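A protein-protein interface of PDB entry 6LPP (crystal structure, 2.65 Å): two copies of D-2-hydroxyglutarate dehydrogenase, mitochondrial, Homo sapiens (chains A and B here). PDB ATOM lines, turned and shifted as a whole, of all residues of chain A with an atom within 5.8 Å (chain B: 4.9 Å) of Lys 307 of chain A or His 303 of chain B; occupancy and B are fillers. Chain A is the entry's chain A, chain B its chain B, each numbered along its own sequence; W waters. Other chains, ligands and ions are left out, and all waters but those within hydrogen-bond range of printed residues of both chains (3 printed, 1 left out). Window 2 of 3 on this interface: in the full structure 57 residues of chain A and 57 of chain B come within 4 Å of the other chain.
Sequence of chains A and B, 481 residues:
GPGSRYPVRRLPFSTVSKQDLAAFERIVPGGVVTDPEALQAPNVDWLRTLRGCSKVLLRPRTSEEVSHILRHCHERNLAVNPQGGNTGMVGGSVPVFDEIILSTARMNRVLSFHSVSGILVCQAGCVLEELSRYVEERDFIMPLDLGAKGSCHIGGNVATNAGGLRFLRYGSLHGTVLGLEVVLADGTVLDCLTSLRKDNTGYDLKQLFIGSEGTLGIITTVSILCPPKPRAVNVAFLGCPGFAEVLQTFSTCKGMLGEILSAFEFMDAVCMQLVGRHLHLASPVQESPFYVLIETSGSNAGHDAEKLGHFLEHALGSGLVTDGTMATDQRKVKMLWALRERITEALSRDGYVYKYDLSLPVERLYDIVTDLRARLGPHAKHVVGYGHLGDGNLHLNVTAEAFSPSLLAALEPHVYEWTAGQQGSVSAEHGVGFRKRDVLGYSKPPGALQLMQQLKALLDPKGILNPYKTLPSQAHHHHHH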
ATOM      1  N   MET A 256     -15.930  21.215 -15.923  1.00  0.00           N
ATOM      2  CA  MET A 256     -15.930  20.038 -15.059  1.00  0.00           C
ATOM      3  C   MET A 256     -16.324  20.321 -13.616  1.00  0.00           C
ATOM      4  O   MET A 256     -16.810  19.411 -12.935  1.00  0.00           O
ATOM      5  CB  MET A 256     -14.549  19.372 -15.086  1.00  0.00           C
ATOM      6  CG  MET A 256     -14.138  18.894 -16.471  1.00  0.00           C
ATOM      7  SD  MET A 256     -12.659  17.863 -16.476  1.00  0.00           S
ATOM      8  CE  MET A 256     -13.312  16.322 -15.840  1.00  0.00           C
ATOM      9  N   LEU A 257     -16.131  21.545 -13.125  1.00  0.00           N
ATOM     10  CA  LEU A 257     -16.547  21.914 -11.777  1.00  0.00           C
ATOM     11  C   LEU A 257     -17.847  22.706 -11.762  1.00  0.00           C
ATOM     12  O   LEU A 257     -18.699  22.473 -10.899  1.00  0.00           O
ATOM     13  CB  LEU A 257     -15.448  22.720 -11.076  1.00  0.00           C
ATOM     14  CG  LEU A 257     -14.077  22.046 -10.948  1.00  0.00           C
ATOM     15  CD1 LEU A 257     -13.108  22.936 -10.186  1.00  0.00           C
ATOM     16  CD2 LEU A 257     -14.196  20.686 -10.274  1.00  0.00           C
ATOM     17  N   GLU A 259     -20.959  24.850 -11.228  1.00  0.00           N
ATOM     18  CA  GLU A 259     -21.595  25.674 -10.206  1.00  0.00           C
ATOM     19  C   GLU A 259     -20.890  25.644  -8.854  1.00  0.00           C
ATOM     20  O   GLU A 259     -21.128  26.539  -8.036  1.00  0.00           O
ATOM     21  CB  GLU A 259     -23.060  25.257 -10.024  1.00  0.00           C
ATOM     22  CG  GLU A 259     -23.284  23.883  -9.387  1.00  0.00           C
ATOM     23  CD  GLU A 259     -22.912  22.723 -10.295  1.00  0.00           C
ATOM     24  OE1 GLU A 259     -22.687  22.951 -11.503  1.00  0.00           O
ATOM     25  OE2 GLU A 259     -22.845  21.579  -9.798  1.00  0.00           O
ATOM     26  N   ILE A 260     -20.037  24.650  -8.583  1.00  0.00           N
ATOM     27  CA  ILE A 260     -19.328  24.662  -7.303  1.00  0.00           C
ATOM     28  C   ILE A 260     -18.122  25.584  -7.304  1.00  0.00           C
ATOM     29  O   ILE A 260     -17.563  25.849  -6.233  1.00  0.00           O
ATOM     30  CB  ILE A 260     -18.872  23.253  -6.875  1.00  0.00           C
ATOM     31  CG1 ILE A 260     -17.779  22.727  -7.806  1.00  0.00           C
ATOM     32  CG2 ILE A 260     -20.058  22.300  -6.829  1.00  0.00           C
ATOM     33  CD1 ILE A 260     -17.090  21.482  -7.285  1.00  0.00           C
ATOM     34  N   GLY A 302     -18.828  15.111  -0.696  1.00  0.00           N
ATOM     35  CA  GLY A 302     -18.430  13.997  -1.539  1.00  0.00           C
ATOM     36  C   GLY A 302     -18.577  14.278  -3.023  1.00  0.00           C
ATOM     37  O   GLY A 302     -17.704  13.919  -3.818  1.00  0.00           O
ATOM     38  N   HIS A 303     -19.676  14.926  -3.417  1.00  0.00           N
ATOM     39  CA  HIS A 303     -19.843  15.301  -4.819  1.00  0.00           C
ATOM     40  C   HIS A 303     -18.759  16.276  -5.262  1.00  0.00           C
ATOM     41  O   HIS A 303     -18.205  16.144  -6.363  1.00  0.00           O
ATOM     42  CB  HIS A 303     -21.234  15.893  -5.037  1.00  0.00           C
ATOM     43  CG  HIS A 303     -22.342  14.899  -4.882  1.00  0.00           C
ATOM     44  ND1 HIS A 303     -23.598  15.244  -4.433  1.00  0.00           N
ATOM     45  CD2 HIS A 303     -22.379  13.565  -5.115  1.00  0.00           C
ATOM     46  CE1 HIS A 303     -24.361  14.167  -4.397  1.00  0.00           C
ATOM     47  NE2 HIS A 303     -23.646  13.135  -4.807  1.00  0.00           N
ATOM     48  N   ASP A 304     -18.443  17.263  -4.421  1.00  0.00           N
ATOM     49  CA  ASP A 304     -17.368  18.197  -4.738  1.00  0.00           C
ATOM     50  C   ASP A 304     -16.041  17.469  -4.898  1.00  0.00           C
ATOM     51  O   ASP A 304     -15.291  17.722  -5.848  1.00  0.00           O
ATOM     52  CB  ASP A 304     -17.253  19.257  -3.644  1.00  0.00           C
ATOM     53  CG  ASP A 304     -18.460  20.160  -3.575  1.00  0.00           C
ATOM     54  OD1 ASP A 304     -19.449  19.902  -4.296  1.00  0.00           O
ATOM     55  OD2 ASP A 304     -18.418  21.128  -2.790  1.00  0.00           O
ATOM     56  N   ALA A 305     -15.707  16.605  -3.937  1.00  0.00           N
ATOM     57  CA  ALA A 305     -14.456  15.856  -4.005  1.00  0.00           C
ATOM     58  C   ALA A 305     -14.377  14.990  -5.257  1.00  0.00           C
ATOM     59  O   ALA A 305     -13.315  14.889  -5.879  1.00  0.00           O
ATOM     60  CB  ALA A 305     -14.294  14.997  -2.750  1.00  0.00           C
ATOM     61  N   GLU A 306     -15.488  14.356  -5.641  1.00  0.00           N
ATOM     62  CA  GLU A 306     -15.517  13.568  -6.873  1.00  0.00           C
ATOM     63  C   GLU A 306     -15.307  14.438  -8.113  1.00  0.00           C
ATOM     64  O   GLU A 306     -14.550  14.065  -9.027  1.00  0.00           O
ATOM     65  CB  GLU A 306     -16.840  12.806  -6.937  1.00  0.00           C
ATOM     66  CG  GLU A 306     -16.890  11.652  -5.936  1.00  0.00           C
ATOM     67  CD  GLU A 306     -18.155  10.822  -6.026  1.00  0.00           C
ATOM     68  OE1 GLU A 306     -18.082   9.666  -6.491  1.00  0.00           O
ATOM     69  OE2 GLU A 306     -19.224  11.326  -5.621  1.00  0.00           O
ATOM     70  N   LYS A 307     -15.953  15.608  -8.154  1.00  0.00           N
ATOM     71  CA  LYS A 307     -15.753  16.524  -9.275  1.00  0.00           C
ATOM     72  C   LYS A 307     -14.293  16.944  -9.365  1.00  0.00           C
ATOM     73  O   LYS A 307     -13.702  16.962 -10.450  1.00  0.00           O
ATOM     74  CB  LYS A 307     -16.656  17.752  -9.143  1.00  0.00           C
ATOM     75  CG  LYS A 307     -18.104  17.539  -9.557  1.00  0.00           C
ATOM     76  CD  LYS A 307     -18.893  18.837  -9.421  1.00  0.00           C
ATOM     77  CE  LYS A 307     -20.286  18.725 -10.025  1.00  0.00           C
ATOM     78  NZ  LYS A 307     -21.284  18.195  -9.058  1.00  0.00           N
ATOM     79  N   LEU A 308     -13.703  17.295  -8.222  1.00  0.00           N
ATOM     80  CA  LEU A 308     -12.298  17.682  -8.192  1.00  0.00           C
ATOM     81  C   LEU A 308     -11.406  16.537  -8.642  1.00  0.00           C
ATOM     82  O   LEU A 308     -10.419  16.757  -9.347  1.00  0.00           O
ATOM     83  CB  LEU A 308     -11.906  18.122  -6.786  1.00  0.00           C
ATOM     84  CG  LEU A 308     -12.130  19.588  -6.447  1.00  0.00           C
ATOM     85  CD1 LEU A 308     -12.066  19.733  -4.955  1.00  0.00           C
ATOM     86  CD2 LEU A 308     -11.088  20.463  -7.120  1.00  0.00           C
ATOM     87  N   GLY A 309     -11.691  15.321  -8.179  1.00  0.00           N
ATOM     88  CA  GLY A 309     -10.906  14.176  -8.604  1.00  0.00           C
ATOM     89  C   GLY A 309     -10.877  14.032 -10.112  1.00  0.00           C
ATOM     90  O   GLY A 309      -9.808  13.918 -10.720  1.00  0.00           O
ATOM     91  N   HIS A 310     -12.058  14.046 -10.739  1.00  0.00           N
ATOM     92  CA  HIS A 310     -12.109  13.908 -12.192  1.00  0.00           C
ATOM     93  C   HIS A 310     -11.437  15.089 -12.892  1.00  0.00           C
ATOM     94  O   HIS A 310     -10.702  14.903 -13.873  1.00  0.00           O
ATOM     95  CB  HIS A 310     -13.564  13.766 -12.649  1.00  0.00           C
ATOM     96  CG  HIS A 310     -13.719  13.248 -14.048  1.00  0.00           C
ATOM     97  ND1 HIS A 310     -14.814  13.544 -14.832  1.00  0.00           N
ATOM     98  CD2 HIS A 310     -12.926  12.444 -14.796  1.00  0.00           C
ATOM     99  CE1 HIS A 310     -14.684  12.953 -16.006  1.00  0.00           C
ATOM    100  NE2 HIS A 310     -13.549  12.278 -16.010  1.00  0.00           N
ATOM    101  N   PHE A 311     -11.626  16.303 -12.364  1.00  0.00           N
ATOM    102  CA  PHE A 311     -10.967  17.481 -12.923  1.00  0.00           C
ATOM    103  C   PHE A 311      -9.448  17.365 -12.874  1.00  0.00           C
ATOM    104  O   PHE A 311      -8.769  17.602 -13.878  1.00  0.00           O
ATOM    105  CB  PHE A 311     -11.432  18.735 -12.182  1.00  0.00           C
ATOM    106  CG  PHE A 311     -10.641  19.963 -12.522  1.00  0.00           C
ATOM    107  CD1 PHE A 311     -10.741  20.550 -13.771  1.00  0.00           C
ATOM    108  CD2 PHE A 311      -9.795  20.532 -11.584  1.00  0.00           C
ATOM    109  CE1 PHE A 311     -10.004  21.678 -14.079  1.00  0.00           C
ATOM    110  CE2 PHE A 311      -9.061  21.659 -11.885  1.00  0.00           C
ATOM    111  CZ  PHE A 311      -9.166  22.235 -13.133  1.00  0.00           C
ATOM    112  N   LEU A 312      -8.896  17.057 -11.699  1.00  0.00           N
ATOM    113  CA  LEU A 312      -7.449  16.931 -11.557  1.00  0.00           C
ATOM    114  C   LEU A 312      -6.907  15.831 -12.455  1.00  0.00           C
ATOM    115  O   LEU A 312      -5.873  16.002 -13.108  1.00  0.00           O
ATOM    116  CB  LEU A 312      -7.061  16.690 -10.097  1.00  0.00           C
ATOM    117  CG  LEU A 312      -7.420  17.810  -9.119  1.00  0.00           C
ATOM    118  CD1 LEU A 312      -7.620  17.268  -7.712  1.00  0.00           C
ATOM    119  CD2 LEU A 312      -6.350  18.894  -9.138  1.00  0.00           C
ATOM    120  N   SER B 299     -23.811  20.804 -13.312  1.00  0.00           N
ATOM    121  CA  SER B 299     -22.810  20.304 -14.246  1.00  0.00           C
ATOM    122  C   SER B 299     -22.777  18.784 -14.332  1.00  0.00           C
ATOM    123  O   SER B 299     -22.377  18.242 -15.368  1.00  0.00           O
ATOM    124  CB  SER B 299     -21.428  20.827 -13.851  1.00  0.00           C
ATOM    125  OG  SER B 299     -20.431  20.357 -14.740  1.00  0.00           O
ATOM    126  N   ASN B 300     -23.170  18.079 -13.274  1.00  0.00           N
ATOM    127  CA  ASN B 300     -23.053  16.624 -13.221  1.00  0.00           C
ATOM    128  C   ASN B 300     -24.433  16.028 -12.974  1.00  0.00           C
ATOM    129  O   ASN B 300     -24.991  16.168 -11.881  1.00  0.00           O
ATOM    130  CB  ASN B 300     -22.063  16.190 -12.140  1.00  0.00           C
ATOM    131  CG  ASN B 300     -21.626  14.747 -12.301  1.00  0.00           C
ATOM    132  OD1 ASN B 300     -22.403  13.822 -12.069  1.00  0.00           O
ATOM    133  ND2 ASN B 300     -20.377  14.548 -12.711  1.00  0.00           N
ATOM    134  N   ALA B 301     -24.976  15.372 -14.003  1.00  0.00           N
ATOM    135  CA  ALA B 301     -26.293  14.746 -13.918  1.00  0.00           C
ATOM    136  C   ALA B 301     -26.397  13.775 -12.745  1.00  0.00           C
ATOM    137  O   ALA B 301     -27.346  13.837 -11.959  1.00  0.00           O
ATOM    138  CB  ALA B 301     -26.616  14.036 -15.233  1.00  0.00           C
ATOM    139  N   GLY B 302     -25.455  12.833 -12.650  1.00  0.00           N
ATOM    140  CA  GLY B 302     -25.445  11.886 -11.540  1.00  0.00           C
ATOM    141  C   GLY B 302     -25.510  12.525 -10.166  1.00  0.00           C
ATOM    142  O   GLY B 302     -26.297  12.110  -9.308  1.00  0.00           O
ATOM    143  N   HIS B 303     -24.692  13.554  -9.937  1.00  0.00           N
ATOM    144  CA  HIS B 303     -24.690  14.214  -8.635  1.00  0.00           C
ATOM    145  C   HIS B 303     -26.011  14.928  -8.371  1.00  0.00           C
ATOM    146  O   HIS B 303     -26.540  14.870  -7.254  1.00  0.00           O
ATOM    147  CB  HIS B 303     -23.517  15.189  -8.549  1.00  0.00           C
ATOM    148  CG  HIS B 303     -22.177  14.526  -8.640  1.00  0.00           C
ATOM    149  ND1 HIS B 303     -21.039  15.193  -9.039  1.00  0.00           N
ATOM    150  CD2 HIS B 303     -21.797  13.250  -8.388  1.00  0.00           C
ATOM    151  CE1 HIS B 303     -20.015  14.360  -9.025  1.00  0.00           C
ATOM    152  NE2 HIS B 303     -20.447  13.174  -8.634  1.00  0.00           N
ATOM    153  N   ASP B 304     -26.546  15.627  -9.374  1.00  0.00           N
ATOM    154  CA  ASP B 304     -27.825  16.307  -9.201  1.00  0.00           C
ATOM    155  C   ASP B 304     -28.938  15.307  -8.914  1.00  0.00           C
ATOM    156  O   ASP B 304     -29.822  15.567  -8.090  1.00  0.00           O
ATOM    157  CB  ASP B 304     -28.154  17.130 -10.444  1.00  0.00           C
ATOM    158  CG  ASP B 304     -27.201  18.285 -10.646  1.00  0.00           C
ATOM    159  OD1 ASP B 304     -26.191  18.360  -9.913  1.00  0.00           O
ATOM    160  OD2 ASP B 304     -27.461  19.118 -11.539  1.00  0.00           O
ATOM    161  N   ALA B 305     -28.909  14.160  -9.596  1.00  0.00           N
ATOM    162  CA  ALA B 305     -29.886  13.105  -9.352  1.00  0.00           C
ATOM    163  C   ALA B 305     -29.787  12.571  -7.929  1.00  0.00           C
ATOM    164  O   ALA B 305     -30.810  12.338  -7.279  1.00  0.00           O
ATOM    165  CB  ALA B 305     -29.701  11.976 -10.365  1.00  0.00           C
ATOM    166  N   GLU B 306     -28.566  12.349  -7.434  1.00  0.00           N
ATOM    167  CA  GLU B 306     -28.399  11.913  -6.048  1.00  0.00           C
ATOM    168  C   GLU B 306     -28.938  12.947  -5.065  1.00  0.00           C
ATOM    169  O   GLU B 306     -29.659  12.610  -4.115  1.00  0.00           O
ATOM    170  CB  GLU B 306     -26.927  11.635  -5.744  1.00  0.00           C
ATOM    171  CG  GLU B 306     -26.534  10.171  -5.726  1.00  0.00           C
ATOM    172  CD  GLU B 306     -25.075   9.975  -5.358  1.00  0.00           C
ATOM    173  OE1 GLU B 306     -24.202  10.202  -6.221  1.00  0.00           O
ATOM    174  OE2 GLU B 306     -24.801   9.613  -4.194  1.00  0.00           O
ATOM    175  N   LYS B 307     -28.587  14.216  -5.282  1.00  0.00           N
ATOM    176  CA  LYS B 307     -29.091  15.299  -4.443  1.00  0.00           C
ATOM    177  C   LYS B 307     -30.617  15.325  -4.411  1.00  0.00           C
ATOM    178  O   LYS B 307     -31.227  15.366  -3.335  1.00  0.00           O
ATOM    179  CB  LYS B 307     -28.552  16.621  -4.993  1.00  0.00           C
ATOM    180  CG  LYS B 307     -27.109  16.944  -4.626  1.00  0.00           C
ATOM    181  CD  LYS B 307     -26.761  18.373  -5.029  1.00  0.00           C
ATOM    182  CE  LYS B 307     -25.367  18.781  -4.575  1.00  0.00           C
ATOM    183  NZ  LYS B 307     -25.259  18.900  -3.100  1.00  0.00           N
HETATM  184  O   HOH W   1     -17.042  14.167 -13.087  1.00  0.00           O
HETATM  185  O   HOH W   2     -18.966  18.260 -13.137  1.00  0.00           O
HETATM  186  O   HOH W   3     -22.030  20.118  -3.342  1.00  0.00           O
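Of the 15 printed residues of chain A, 4 touch a printed residue of chain B.
Hydrophobic or aromatic side chains of chain A that line the printed part of chain B: His 303.
Along chain A the printed residues that touch a printed residue of chain B span positions 259 to 307.
Of the 9 printed residues of chain B, 5 touch a printed residue of chain A.
Hydrophobic or aromatic side chains of chain B that line the printed part of chain A: His 303.
Among the printed residues, 7 pairs touch across the chains.
Among the printed residues, no Asp or Glu carboxylate lies within 4 Å of a Lys or Arg side-chain nitrogen of the other chain.
His 303 of chain B touches its own counterpart, His 303 of chain A.
His 303 of chain A touches Glu 306 of chain B, and with the chains exchanged Glu 306 of chain A touches His 303 of chain B.
His 303 of chain A touches Lys 307 of chain B, and with the chains exchanged Lys 307 of chain A touches His 303 of chain B.
Of the 7 pairs that touch across the chains among the printed residues, 5 have their exchanged pair printed and touching as well.
Lys 307 of chain A touches just these residues of chain B: Asn 300 and His 303.
Of chain A, only His 303, Glu 306 and Lys 307 come within 4 Å of His 303 of chain B.
Of the printed residues of chain A, Lys 307 of chain B touches His 303 (3.9 Å).
Printed residues of chain A within 4 Å of Asn 300 of chain B: Lys 307.
Of the printed residues of chain B, His 303 of chain A touches His 303, Glu 306 and Lys 307.
The nearest residue of chain B that does not touch Lys 307 of chain A is Ser 299 of chain B (4.5 Å).
The side-chain carboxylate of Glu 259 of chain A lies within salt-bridge range of the side-chain amino group of Lys 307 of chain A, 3.8 Å away.
The side-chain amide oxygen (OD1) of Asn 300 of chain B lies within hydrogen-bond range of the backbone NH (N) of Gly 302 of chain B (3.3 Å).
The backbone NH (N) of His 303 of chain B is in hydrogen-bond range of the side-chain amide oxygen (OD1) of Asn 300 of chain B (3.1 Å).
His 303 of chain A touches His 303 of chain B (CD2 to CD2, 3.3 Å).
Lys 307 of chain B touches His 303 of chain A (CG to ND1, 3.9 Å).
NE2 of His 303 of chain B touches OE2 of Glu 306 of chain A (3.7 Å).
Lys 307 of chain A touches Asn 300 of chain B.
OE1 of Glu 259 of chain A is in hydrogen-bond range of N of Ser 299 of chain B (3.0 Å).
OE1 of Glu 306 of chain B lies within hydrogen-bond range of NE2 of His 303 of chain A (3.3 Å).
A ring nitrogen (ND1) of His 303 of chain B sits at hydrogen-bond distance from the side-chain amino group (NZ) of Lys 307 of chain A (3.0 Å).
Water W2 bridges O of Met 256 of chain A (2.5 Å) and OG of Ser 299 of chain B (3.0 Å).
Water W3 bridges OD1 of Asp 304 of chain A (2.8 Å) and NZ of Lys 307 of chain B (3.5 Å).
Water W1 lies within hydrogen-bond range of a ring nitrogen (ND1) of His 310 of chain A (2.9 Å) and the side-chain amide nitrogen (ND2) of Asn 300 of chain B (3.4 Å).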
